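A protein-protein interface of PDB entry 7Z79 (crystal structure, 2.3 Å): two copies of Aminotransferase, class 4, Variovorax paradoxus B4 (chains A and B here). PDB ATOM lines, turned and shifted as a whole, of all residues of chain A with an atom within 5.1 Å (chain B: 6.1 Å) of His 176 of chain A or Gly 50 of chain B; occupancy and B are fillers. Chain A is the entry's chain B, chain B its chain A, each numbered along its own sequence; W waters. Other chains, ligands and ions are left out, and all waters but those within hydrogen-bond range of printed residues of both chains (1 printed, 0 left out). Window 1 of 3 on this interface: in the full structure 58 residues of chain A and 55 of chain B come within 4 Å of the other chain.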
ATOM      1  N   GLY A  46       9.588  23.128  -5.590  1.00  0.00           N
ATOM      2  CA  GLY A  46      10.919  22.770  -6.029  1.00  0.00           C
ATOM      3  C   GLY A  46      11.855  23.973  -5.966  1.00  0.00           C
ATOM      4  O   GLY A  46      12.968  23.820  -5.443  1.00  0.00           O
ATOM      5  N   GLY A  50      13.461  23.188  -2.598  1.00  0.00           N
ATOM      6  CA  GLY A  50      14.122  21.969  -3.005  1.00  0.00           C
ATOM      7  C   GLY A  50      13.250  20.750  -2.745  1.00  0.00           C
ATOM      8  O   GLY A  50      13.793  19.671  -2.487  1.00  0.00           O
ATOM      9  N   ASP A  51      11.918  20.940  -2.873  1.00  0.00           N
ATOM     10  CA  ASP A  51      10.959  19.949  -2.421  1.00  0.00           C
ATOM     11  C   ASP A  51      10.461  19.158  -3.616  1.00  0.00           C
ATOM     12  O   ASP A  51       9.422  19.485  -4.200  1.00  0.00           O
ATOM     13  CB  ASP A  51       9.846  20.599  -1.621  1.00  0.00           C
ATOM     14  CG  ASP A  51       8.794  19.634  -1.076  1.00  0.00           C
ATOM     15  OD1 ASP A  51       8.962  18.393  -1.235  1.00  0.00           O
ATOM     16  OD2 ASP A  51       7.793  20.151  -0.501  1.00  0.00           O
ATOM     17  N   GLY A  52      11.190  18.084  -3.973  1.00  0.00           N
ATOM     18  CA  GLY A  52      10.809  17.209  -5.070  1.00  0.00           C
ATOM     19  C   GLY A  52      11.789  16.053  -5.193  1.00  0.00           C
ATOM     20  O   GLY A  52      12.795  16.028  -4.470  1.00  0.00           O
ATOM     21  N   VAL A  53      11.485  15.100  -6.104  1.00  0.00           N
ATOM     22  CA  VAL A  53      12.406  14.005  -6.370  1.00  0.00           C
ATOM     23  C   VAL A  53      12.621  13.988  -7.877  1.00  0.00           C
ATOM     24  O   VAL A  53      11.749  14.478  -8.639  1.00  0.00           O
ATOM     25  CB  VAL A  53      11.834  12.668  -5.861  1.00  0.00           C
ATOM     26  CG1 VAL A  53      11.858  12.597  -4.330  1.00  0.00           C
ATOM     27  CG2 VAL A  53      10.432  12.386  -6.409  1.00  0.00           C
ATOM     28  N   TRP A  54      13.767  13.430  -8.310  1.00  0.00           N
ATOM     29  CA  TRP A  54      14.110  13.382  -9.724  1.00  0.00           C
ATOM     30  C   TRP A  54      14.807  12.077 -10.060  1.00  0.00           C
ATOM     31  O   TRP A  54      15.280  11.368  -9.196  1.00  0.00           O
ATOM     32  CB  TRP A  54      14.931  14.600 -10.095  1.00  0.00           C
ATOM     33  CG  TRP A  54      16.270  14.567  -9.407  1.00  0.00           C
ATOM     34  CD1 TRP A  54      16.524  14.994  -8.129  1.00  0.00           C
ATOM     35  CD2 TRP A  54      17.500  14.024  -9.936  1.00  0.00           C
ATOM     36  NE1 TRP A  54      17.813  14.744  -7.838  1.00  0.00           N
ATOM     37  CE2 TRP A  54      18.441  14.141  -8.899  1.00  0.00           C
ATOM     38  CE3 TRP A  54      17.895  13.424 -11.140  1.00  0.00           C
ATOM     39  CZ2 TRP A  54      19.791  13.730  -9.055  1.00  0.00           C
ATOM     40  CZ3 TRP A  54      19.194  13.003 -11.309  1.00  0.00           C
ATOM     41  CH2 TRP A  54      20.147  13.145 -10.276  1.00  0.00           C
ATOM     42  N   MET A 114      11.951  15.556 -13.332  1.00  0.00           N
ATOM     43  CA  MET A 114      11.857  16.290 -12.086  1.00  0.00           C
ATOM     44  C   MET A 114      10.398  16.466 -11.679  1.00  0.00           C
ATOM     45  O   MET A 114       9.570  16.932 -12.486  1.00  0.00           O
ATOM     46  CB  MET A 114      12.538  17.658 -12.245  1.00  0.00           C
ATOM     47  CG  MET A 114      14.078  17.511 -12.379  1.00  0.00           C
ATOM     48  SD  MET A 114      14.844  19.098 -12.701  1.00  0.00           S
ATOM     49  CE  MET A 114      14.394  19.439 -14.425  1.00  0.00           C
ATOM     50  N   VAL A 115      10.088  16.022 -10.455  1.00  0.00           N
ATOM     51  CA  VAL A 115       8.719  16.075  -9.935  1.00  0.00           C
ATOM     52  C   VAL A 115       8.817  16.791  -8.585  1.00  0.00           C
ATOM     53  O   VAL A 115       9.399  16.255  -7.618  1.00  0.00           O
ATOM     54  CB  VAL A 115       8.097  14.681  -9.765  1.00  0.00           C
ATOM     55  CG1 VAL A 115       6.699  14.773  -9.217  1.00  0.00           C
ATOM     56  CG2 VAL A 115       8.051  13.889 -11.082  1.00  0.00           C
ATOM     57  N   THR A 116       8.233  17.986  -8.531  1.00  0.00           N
ATOM     58  CA  THR A 116       8.257  18.782  -7.324  1.00  0.00           C
ATOM     59  C   THR A 116       6.843  18.871  -6.773  1.00  0.00           C
ATOM     60  O   THR A 116       5.903  18.628  -7.518  1.00  0.00           O
ATOM     61  CB  THR A 116       8.986  20.116  -7.622  1.00  0.00           C
ATOM     62  OG1 THR A 116       8.289  20.840  -8.662  1.00  0.00           O
ATOM     63  CG2 THR A 116      10.472  19.884  -7.910  1.00  0.00           C
ATOM     64  N   ASN A 174      16.625  10.826  -3.851  1.00  0.00           N
ATOM     65  CA  ASN A 174      17.169  11.557  -4.980  1.00  0.00           C
ATOM     66  C   ASN A 174      16.296  12.803  -5.138  1.00  0.00           C
ATOM     67  O   ASN A 174      15.329  12.817  -5.902  1.00  0.00           O
ATOM     68  CB  ASN A 174      17.164  10.683  -6.262  1.00  0.00           C
ATOM     69  CG  ASN A 174      18.277  11.040  -7.244  1.00  0.00           C
ATOM     70  OD1 ASN A 174      19.406  11.281  -6.853  1.00  0.00           O
ATOM     71  ND2 ASN A 174      17.995  11.051  -8.531  1.00  0.00           N
ATOM     72  N   SER A 175      16.655  13.862  -4.413  1.00  0.00           N
ATOM     73  CA  SER A 175      15.752  14.990  -4.183  1.00  0.00           C
ATOM     74  C   SER A 175      16.328  16.249  -4.798  1.00  0.00           C
ATOM     75  O   SER A 175      17.520  16.281  -5.158  1.00  0.00           O
ATOM     76  CB  SER A 175      15.491  15.219  -2.678  1.00  0.00           C
ATOM     77  OG  SER A 175      16.550  15.988  -2.098  1.00  0.00           O
ATOM     78  N   HIS A 176      15.467  17.293  -4.786  1.00  0.00           N
ATOM     79  CA  HIS A 176      15.818  18.631  -5.210  1.00  0.00           C
ATOM     80  C   HIS A 176      16.527  19.406  -4.117  1.00  0.00           C
ATOM     81  O   HIS A 176      16.814  20.590  -4.344  1.00  0.00           O
ATOM     82  CB  HIS A 176      14.582  19.366  -5.717  1.00  0.00           C
ATOM     83  CG  HIS A 176      14.165  18.866  -7.056  1.00  0.00           C
ATOM     84  ND1 HIS A 176      14.197  19.687  -8.168  1.00  0.00           N
ATOM     85  CD2 HIS A 176      13.766  17.639  -7.475  1.00  0.00           C
ATOM     86  CE1 HIS A 176      13.757  19.031  -9.243  1.00  0.00           C
ATOM     87  NE2 HIS A 176      13.539  17.726  -8.845  1.00  0.00           N
ATOM     88  N   SER A 177      16.792  18.780  -2.945  1.00  0.00           N
ATOM     89  CA  SER A 177      17.510  19.418  -1.866  1.00  0.00           C
ATOM     90  C   SER A 177      18.967  18.939  -1.915  1.00  0.00           C
ATOM     91  O   SER A 177      19.335  17.961  -1.261  1.00  0.00           O
ATOM     92  CB  SER A 177      16.844  19.171  -0.527  1.00  0.00           C
ATOM     93  OG  SER A 177      15.645  20.002  -0.393  1.00  0.00           O
ATOM     94  N   ARG A 178      19.827  19.650  -2.665  1.00  0.00           N
ATOM     95  CA  ARG A 178      21.121  19.081  -3.035  1.00  0.00           C
ATOM     96  C   ARG A 178      22.273  19.906  -2.450  1.00  0.00           C
ATOM     97  O   ARG A 178      23.416  19.541  -2.725  1.00  0.00           O
ATOM     98  CB  ARG A 178      21.235  18.889  -4.538  1.00  0.00           C
ATOM     99  CG  ARG A 178      20.012  18.183  -5.144  1.00  0.00           C
ATOM    100  CD  ARG A 178      20.221  17.654  -6.563  1.00  0.00           C
ATOM    101  NE  ARG A 178      21.214  16.585  -6.762  1.00  0.00           N
ATOM    102  CZ  ARG A 178      21.156  15.352  -6.200  1.00  0.00           C
ATOM    103  NH1 ARG A 178      20.183  14.996  -5.347  1.00  0.00           N
ATOM    104  NH2 ARG A 178      22.064  14.467  -6.548  1.00  0.00           N
ATOM    105  N   LEU A 179      22.014  20.969  -1.620  1.00  0.00           N
ATOM    106  CA  LEU A 179      23.170  21.686  -1.082  1.00  0.00           C
ATOM    107  C   LEU A 179      24.038  20.798  -0.196  1.00  0.00           C
ATOM    108  O   LEU A 179      25.223  21.091  -0.055  1.00  0.00           O
ATOM    109  CB  LEU A 179      22.811  22.969  -0.336  1.00  0.00           C
ATOM    110  CG  LEU A 179      22.501  24.158  -1.223  1.00  0.00           C
ATOM    111  CD1 LEU A 179      21.818  25.174  -0.314  1.00  0.00           C
ATOM    112  CD2 LEU A 179      23.827  24.689  -1.725  1.00  0.00           C
ATOM    113  N   ALA B  45      19.287  26.887 -10.763  1.00  0.00           N
ATOM    114  CA  ALA B  45      19.902  26.153  -9.673  1.00  0.00           C
ATOM    115  C   ALA B  45      18.961  25.984  -8.470  1.00  0.00           C
ATOM    116  O   ALA B  45      19.001  24.940  -7.790  1.00  0.00           O
ATOM    117  CB  ALA B  45      21.237  26.762  -9.304  1.00  0.00           C
ATOM    118  N   GLY B  46      18.100  27.016  -8.225  1.00  0.00           N
ATOM    119  CA  GLY B  46      17.135  26.983  -7.146  1.00  0.00           C
ATOM    120  C   GLY B  46      16.150  25.821  -7.337  1.00  0.00           C
ATOM    121  O   GLY B  46      15.869  25.072  -6.388  1.00  0.00           O
ATOM    122  N   TYR B  47      15.607  25.721  -8.539  1.00  0.00           N
ATOM    123  CA  TYR B  47      14.606  24.672  -8.804  1.00  0.00           C
ATOM    124  C   TYR B  47      15.282  23.321  -8.937  1.00  0.00           C
ATOM    125  O   TYR B  47      14.724  22.386  -8.398  1.00  0.00           O
ATOM    126  CB  TYR B  47      13.808  24.980 -10.070  1.00  0.00           C
ATOM    127  CG  TYR B  47      12.845  23.897 -10.482  1.00  0.00           C
ATOM    128  CD1 TYR B  47      13.120  23.048 -11.540  1.00  0.00           C
ATOM    129  CD2 TYR B  47      11.662  23.710  -9.795  1.00  0.00           C
ATOM    130  CE1 TYR B  47      12.243  22.042 -11.906  1.00  0.00           C
ATOM    131  CE2 TYR B  47      10.772  22.714 -10.151  1.00  0.00           C
ATOM    132  CZ  TYR B  47      11.062  21.876 -11.209  1.00  0.00           C
ATOM    133  OH  TYR B  47      10.179  20.896 -11.549  1.00  0.00           O
ATOM    134  N   VAL B  48      16.469  23.251  -9.545  1.00  0.00           N
ATOM    135  CA  VAL B  48      16.982  21.909  -9.823  1.00  0.00           C
ATOM    136  C   VAL B  48      17.549  21.260  -8.562  1.00  0.00           C
ATOM    137  O   VAL B  48      17.420  20.043  -8.410  1.00  0.00           O
ATOM    138  CB  VAL B  48      18.031  21.874 -10.977  1.00  0.00           C
ATOM    139  CG1 VAL B  48      18.626  20.478 -11.198  1.00  0.00           C
ATOM    140  CG2 VAL B  48      17.448  22.452 -12.278  1.00  0.00           C
ATOM    141  N   CYS B  49      18.111  22.090  -7.655  1.00  0.00           N
ATOM    142  CA  CYS B  49      19.080  21.664  -6.684  1.00  0.00           C
ATOM    143  C   CYS B  49      18.830  22.301  -5.314  1.00  0.00           C
ATOM    144  O   CYS B  49      19.596  21.973  -4.379  1.00  0.00           O
ATOM    145  CB  CYS B  49      20.435  22.206  -7.121  1.00  0.00           C
ATOM    146  SG  CYS B  49      21.135  21.179  -8.397  1.00  0.00           S
ATOM    147  N   GLY B  50      17.825  23.187  -5.185  1.00  0.00           N
ATOM    148  CA  GLY B  50      17.628  23.887  -3.936  1.00  0.00           C
ATOM    149  C   GLY B  50      18.848  24.745  -3.622  1.00  0.00           C
ATOM    150  O   GLY B  50      19.194  24.920  -2.445  1.00  0.00           O
ATOM    151  N   ASP B  51      19.460  25.299  -4.685  1.00  0.00           N
ATOM    152  CA  ASP B  51      20.764  25.923  -4.558  1.00  0.00           C
ATOM    153  C   ASP B  51      20.590  27.440  -4.493  1.00  0.00           C
ATOM    154  O   ASP B  51      20.653  28.122  -5.523  1.00  0.00           O
ATOM    155  CB  ASP B  51      21.703  25.442  -5.662  1.00  0.00           C
ATOM    156  CG  ASP B  51      23.106  26.018  -5.609  1.00  0.00           C
ATOM    157  OD1 ASP B  51      23.477  26.702  -4.616  1.00  0.00           O
ATOM    158  OD2 ASP B  51      23.824  25.747  -6.537  1.00  0.00           O
ATOM    159  N   GLY B  52      20.449  27.973  -3.270  1.00  0.00           N
ATOM    160  CA  GLY B  52      20.203  29.390  -3.085  1.00  0.00           C
ATOM    161  C   GLY B  52      20.032  29.736  -1.606  1.00  0.00           C
ATOM    162  O   GLY B  52      19.944  28.812  -0.808  1.00  0.00           O
ATOM    163  N   THR B 116      19.142  32.553  -5.892  1.00  0.00           N
ATOM    164  CA  THR B 116      19.563  31.211  -6.287  1.00  0.00           C
ATOM    165  C   THR B 116      20.748  31.350  -7.234  1.00  0.00           C
ATOM    166  O   THR B 116      20.941  32.439  -7.765  1.00  0.00           O
ATOM    167  CB  THR B 116      18.381  30.385  -6.765  1.00  0.00           C
ATOM    168  OG1 THR B 116      17.789  31.044  -7.886  1.00  0.00           O
ATOM    169  CG2 THR B 116      17.385  30.126  -5.654  1.00  0.00           C
ATOM    170  N   SER B 175      18.623  28.292   3.391  1.00  0.00           N
ATOM    171  CA  SER B 175      18.825  27.900   2.002  1.00  0.00           C
ATOM    172  C   SER B 175      17.538  27.395   1.380  1.00  0.00           C
ATOM    173  O   SER B 175      16.549  27.165   2.085  1.00  0.00           O
ATOM    174  CB  SER B 175      19.860  26.810   1.879  1.00  0.00           C
ATOM    175  OG  SER B 175      19.316  25.505   2.121  1.00  0.00           O
ATOM    176  N   HIS B 176      17.629  27.149   0.049  1.00  0.00           N
ATOM    177  CA  HIS B 176      16.564  26.584  -0.733  1.00  0.00           C
ATOM    178  C   HIS B 176      16.545  25.063  -0.638  1.00  0.00           C
ATOM    179  O   HIS B 176      15.710  24.449  -1.304  1.00  0.00           O
ATOM    180  CB  HIS B 176      16.642  27.083  -2.165  1.00  0.00           C
ATOM    181  CG  HIS B 176      16.162  28.489  -2.287  1.00  0.00           C
ATOM    182  ND1 HIS B 176      15.088  28.813  -3.055  1.00  0.00           N
ATOM    183  CD2 HIS B 176      16.634  29.651  -1.750  1.00  0.00           C
ATOM    184  CE1 HIS B 176      14.900  30.139  -3.000  1.00  0.00           C
ATOM    185  NE2 HIS B 176      15.848  30.675  -2.177  1.00  0.00           N
ATOM    186  N   SER B 177      17.429  24.452   0.166  1.00  0.00           N
ATOM    187  CA  SER B 177      17.442  23.002   0.305  1.00  0.00           C
ATOM    188  C   SER B 177      16.770  22.648   1.626  1.00  0.00           C
ATOM    189  O   SER B 177      17.442  22.560   2.660  1.00  0.00           O
ATOM    190  CB  SER B 177      18.905  22.492   0.272  1.00  0.00           C
ATOM    191  OG  SER B 177      19.360  22.443  -1.085  1.00  0.00           O
ATOM    192  N   ARG B 178      15.442  22.435   1.625  1.00  0.00           N
ATOM    193  CA  ARG B 178      14.680  22.509   2.890  1.00  0.00           C
ATOM    194  C   ARG B 178      14.014  21.174   3.212  1.00  0.00           C
ATOM    195  O   ARG B 178      13.285  21.085   4.177  1.00  0.00           O
ATOM    196  CB  ARG B 178      13.645  23.620   2.846  1.00  0.00           C
ATOM    197  CG  ARG B 178      14.284  24.953   2.476  1.00  0.00           C
ATOM    198  CD  ARG B 178      13.419  26.176   2.784  1.00  0.00           C
ATOM    199  NE  ARG B 178      13.141  26.473   4.167  1.00  0.00           N
ATOM    200  CZ  ARG B 178      14.066  26.808   5.112  1.00  0.00           C
ATOM    201  NH1 ARG B 178      15.366  26.806   4.790  1.00  0.00           N
ATOM    202  NH2 ARG B 178      13.672  27.181   6.359  1.00  0.00           N
ATOM    203  N   LEU B 179      14.262  20.116   2.430  1.00  0.00           N
ATOM    204  CA  LEU B 179      13.708  18.811   2.716  1.00  0.00           C
ATOM    205  C   LEU B 179      14.187  18.316   4.098  1.00  0.00           C
ATOM    206  O   LEU B 179      13.440  17.540   4.730  1.00  0.00           O
ATOM    207  CB  LEU B 179      14.041  17.806   1.599  1.00  0.00           C
ATOM    208  CG  LEU B 179      13.023  17.876   0.469  1.00  0.00           C
ATOM    209  CD1 LEU B 179      13.491  17.025  -0.692  1.00  0.00           C
ATOM    210  CD2 LEU B 179      11.622  17.372   0.876  1.00  0.00           C
HETATM  211  O   HOH W   1      16.904  17.879  -9.635  1.00  0.00           O
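Of chain B, only Tyr 47, Val 48, Cys 49 and Gly 50 come within 4 Å of His 176 of chain A.
Of chain A, only His 176 and Leu 179 come within 4 Å of Gly 50 of chain B.
Printed residues of chain A within 4 Å of Leu 179 of chain B: Gly 50 (3.2 Å), Asp 51 (3.5 Å), Gly 52 (3.97 Å), Ser 175 (3.3 Å) and Ser 177 (3.1 Å).
Of the printed residues of chain A, Val 48 of chain B touches His 176 (3.3 Å).
Printed residues of chain A within 4 Å of Gly 46 of chain B: Gly 46 (3.3 Å).
Printed residues of chain A within 4 Å of His 176 of chain B: Gly 50.
Of the printed residues of chain B, Asp 51 of chain A touches Leu 179 (3.5 Å).
Ala 45 of chain B touches none of the printed residues of chain A.
Val 115 of chain A touches none of the printed residues of chain B.
The nearest printed residue of chain B that does not touch His 176 of chain A is Ser 177 of chain B (4.5 Å).
Water W1 lies within hydrogen-bond range of the backbone carbonyl oxygen of Val 48 of chain B and a ring nitrogen (NE2) of His 176 of chain A.
Of the 14 printed residues of chain B, 11 touch a printed residue of chain A.
Hydrophobic or aromatic side chains of chain B that line the printed part of chain A: Tyr 47 and Leu 179.
Along chain B the printed residues that touch a printed residue of chain A span positions 46 to 179.
Of the 15 printed residues of chain A, 10 touch a printed residue of chain B.
Hydrophobic or aromatic side chains of chain A that line the printed part of chain B: His 176 and Leu 179.
Among the printed residues, no Asp or Glu carboxylate lies within 4 Å of a Lys or Arg side-chain nitrogen of the other chain.
Gly 46 of chain A touches Tyr 47 of chain B.
Gly 50 of chain A touches Leu 179 of chain B.
Asp 51 of chain A touches Leu 179 of chain B.
Leu 179 of chain B touches Gly 52 of chain A (CD1 to O, 3.97 Å).
Ser 175 of chain A touches Leu 179 of chain B.
OG of Ser 177 of chain A touches C of Ser 177 of chain B, 3.5 Å away.
Cys 49 of chain B touches Leu 179 of chain A.
Gly 50 of chain B touches Leu 179 of chain A.
Asp 51 of chain B touches Leu 179 of chain A (OD1 to CD2, 3.5 Å).
Leu 179 of chain A touches Ser 175 of chain B (CD1 to CB, 3.4 Å).
Gly 50 of chain A touches His 176 of chain B, and with the chains exchanged His 176 of chain A touches Gly 50 of chain B.
Gly 52 of chain A touches Leu 179 of chain B, but with the chains exchanged Leu 179 of chain A does not touch Gly 52 of chain B (4.1 Å).
Ser 175 of chain A touches Leu 179 of chain B, and with the chains exchanged Leu 179 of chain A touches Ser 175 of chain B.
Ser 177 of chain B touches its own counterpart, Ser 177 of chain A.
10 positions are printed for both chains.
Of the 23 pairs that touch across the chains among the printed residues, 14 have their exchanged pair printed and touching as well.
The side-chain hydroxyl (OG1) of Thr 116 of chain A lies close to the side-chain hydroxyl (OH) of Tyr 47 of chain B.
ND1 of His 176 of chain A is in hydrogen-bond range of O of Tyr 47 of chain B (2.8 Å).
The backbone carbonyl oxygen (O) of Val 48 of chain B sits at hydrogen-bond distance from a ring nitrogen (ND1) of His 176 of chain A, at 3.3 Å.
The backbone carbonyl oxygen (O) of Cys 49 of chain B is in hydrogen-bond range of the backbone NH (N) of Arg 178 of chain A, 2.9 Å away.
N of Gly 50 of chain B is in hydrogen-bond range of O of His 176 of chain A, 2.9 Å away.
O of His 176 of chain B lies within hydrogen-bond range of N of Gly 50 of chain A (2.9 Å).
The side-chain hydroxyl of Ser 177 of chain B sits at hydrogen-bond distance from the backbone NH of Arg 178 of chain A, 3.2 Å away.
The backbone NH of Leu 179 of chain A sits at hydrogen-bond distance from the side-chain hydroxyl of Ser 177 of chain B (3.1 Å).
The side-chain hydroxyl of Ser 177 of chain A is in hydrogen-bond range of the backbone NH of Arg 178 of chain B, 3.2 Å away.
OG of Ser 177 of chain A sits at hydrogen-bond distance from N of Leu 179 of chain B (3.1 Å).
O of Gly 46 of chain B sits close to O of Gly 46 of chain A, at 3.3 Å.
The backbone carbonyl oxygen (O) of His 176 of chain A lies close to the backbone carbonyl oxygen (O) of Cys 49 of chain B.
O of Ala 45 of chain B is in hydrogen-bond range of N of Gly 50 of chain B, at 3.4 Å.
The backbone carbonyl oxygen of Cys 49 of chain B is in hydrogen-bond range of the side-chain hydroxyl of Ser 177 of chain B.
The backbone carbonyl oxygen of Gly 50 of chain B sits at hydrogen-bond distance from the side-chain hydroxyl of Ser 177 of chain B.
O of Gly 52 of chain B sits at hydrogen-bond distance from N of His 176 of chain B (3.0 Å).
The backbone carbonyl oxygen of Gly 52 of chain A is in hydrogen-bond range of the backbone NH of His 176 of chain A (3.0 Å).
O of Ser 175 of chain A lies within hydrogen-bond range of NE1 of Trp 54 of chain A (3.1 Å).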
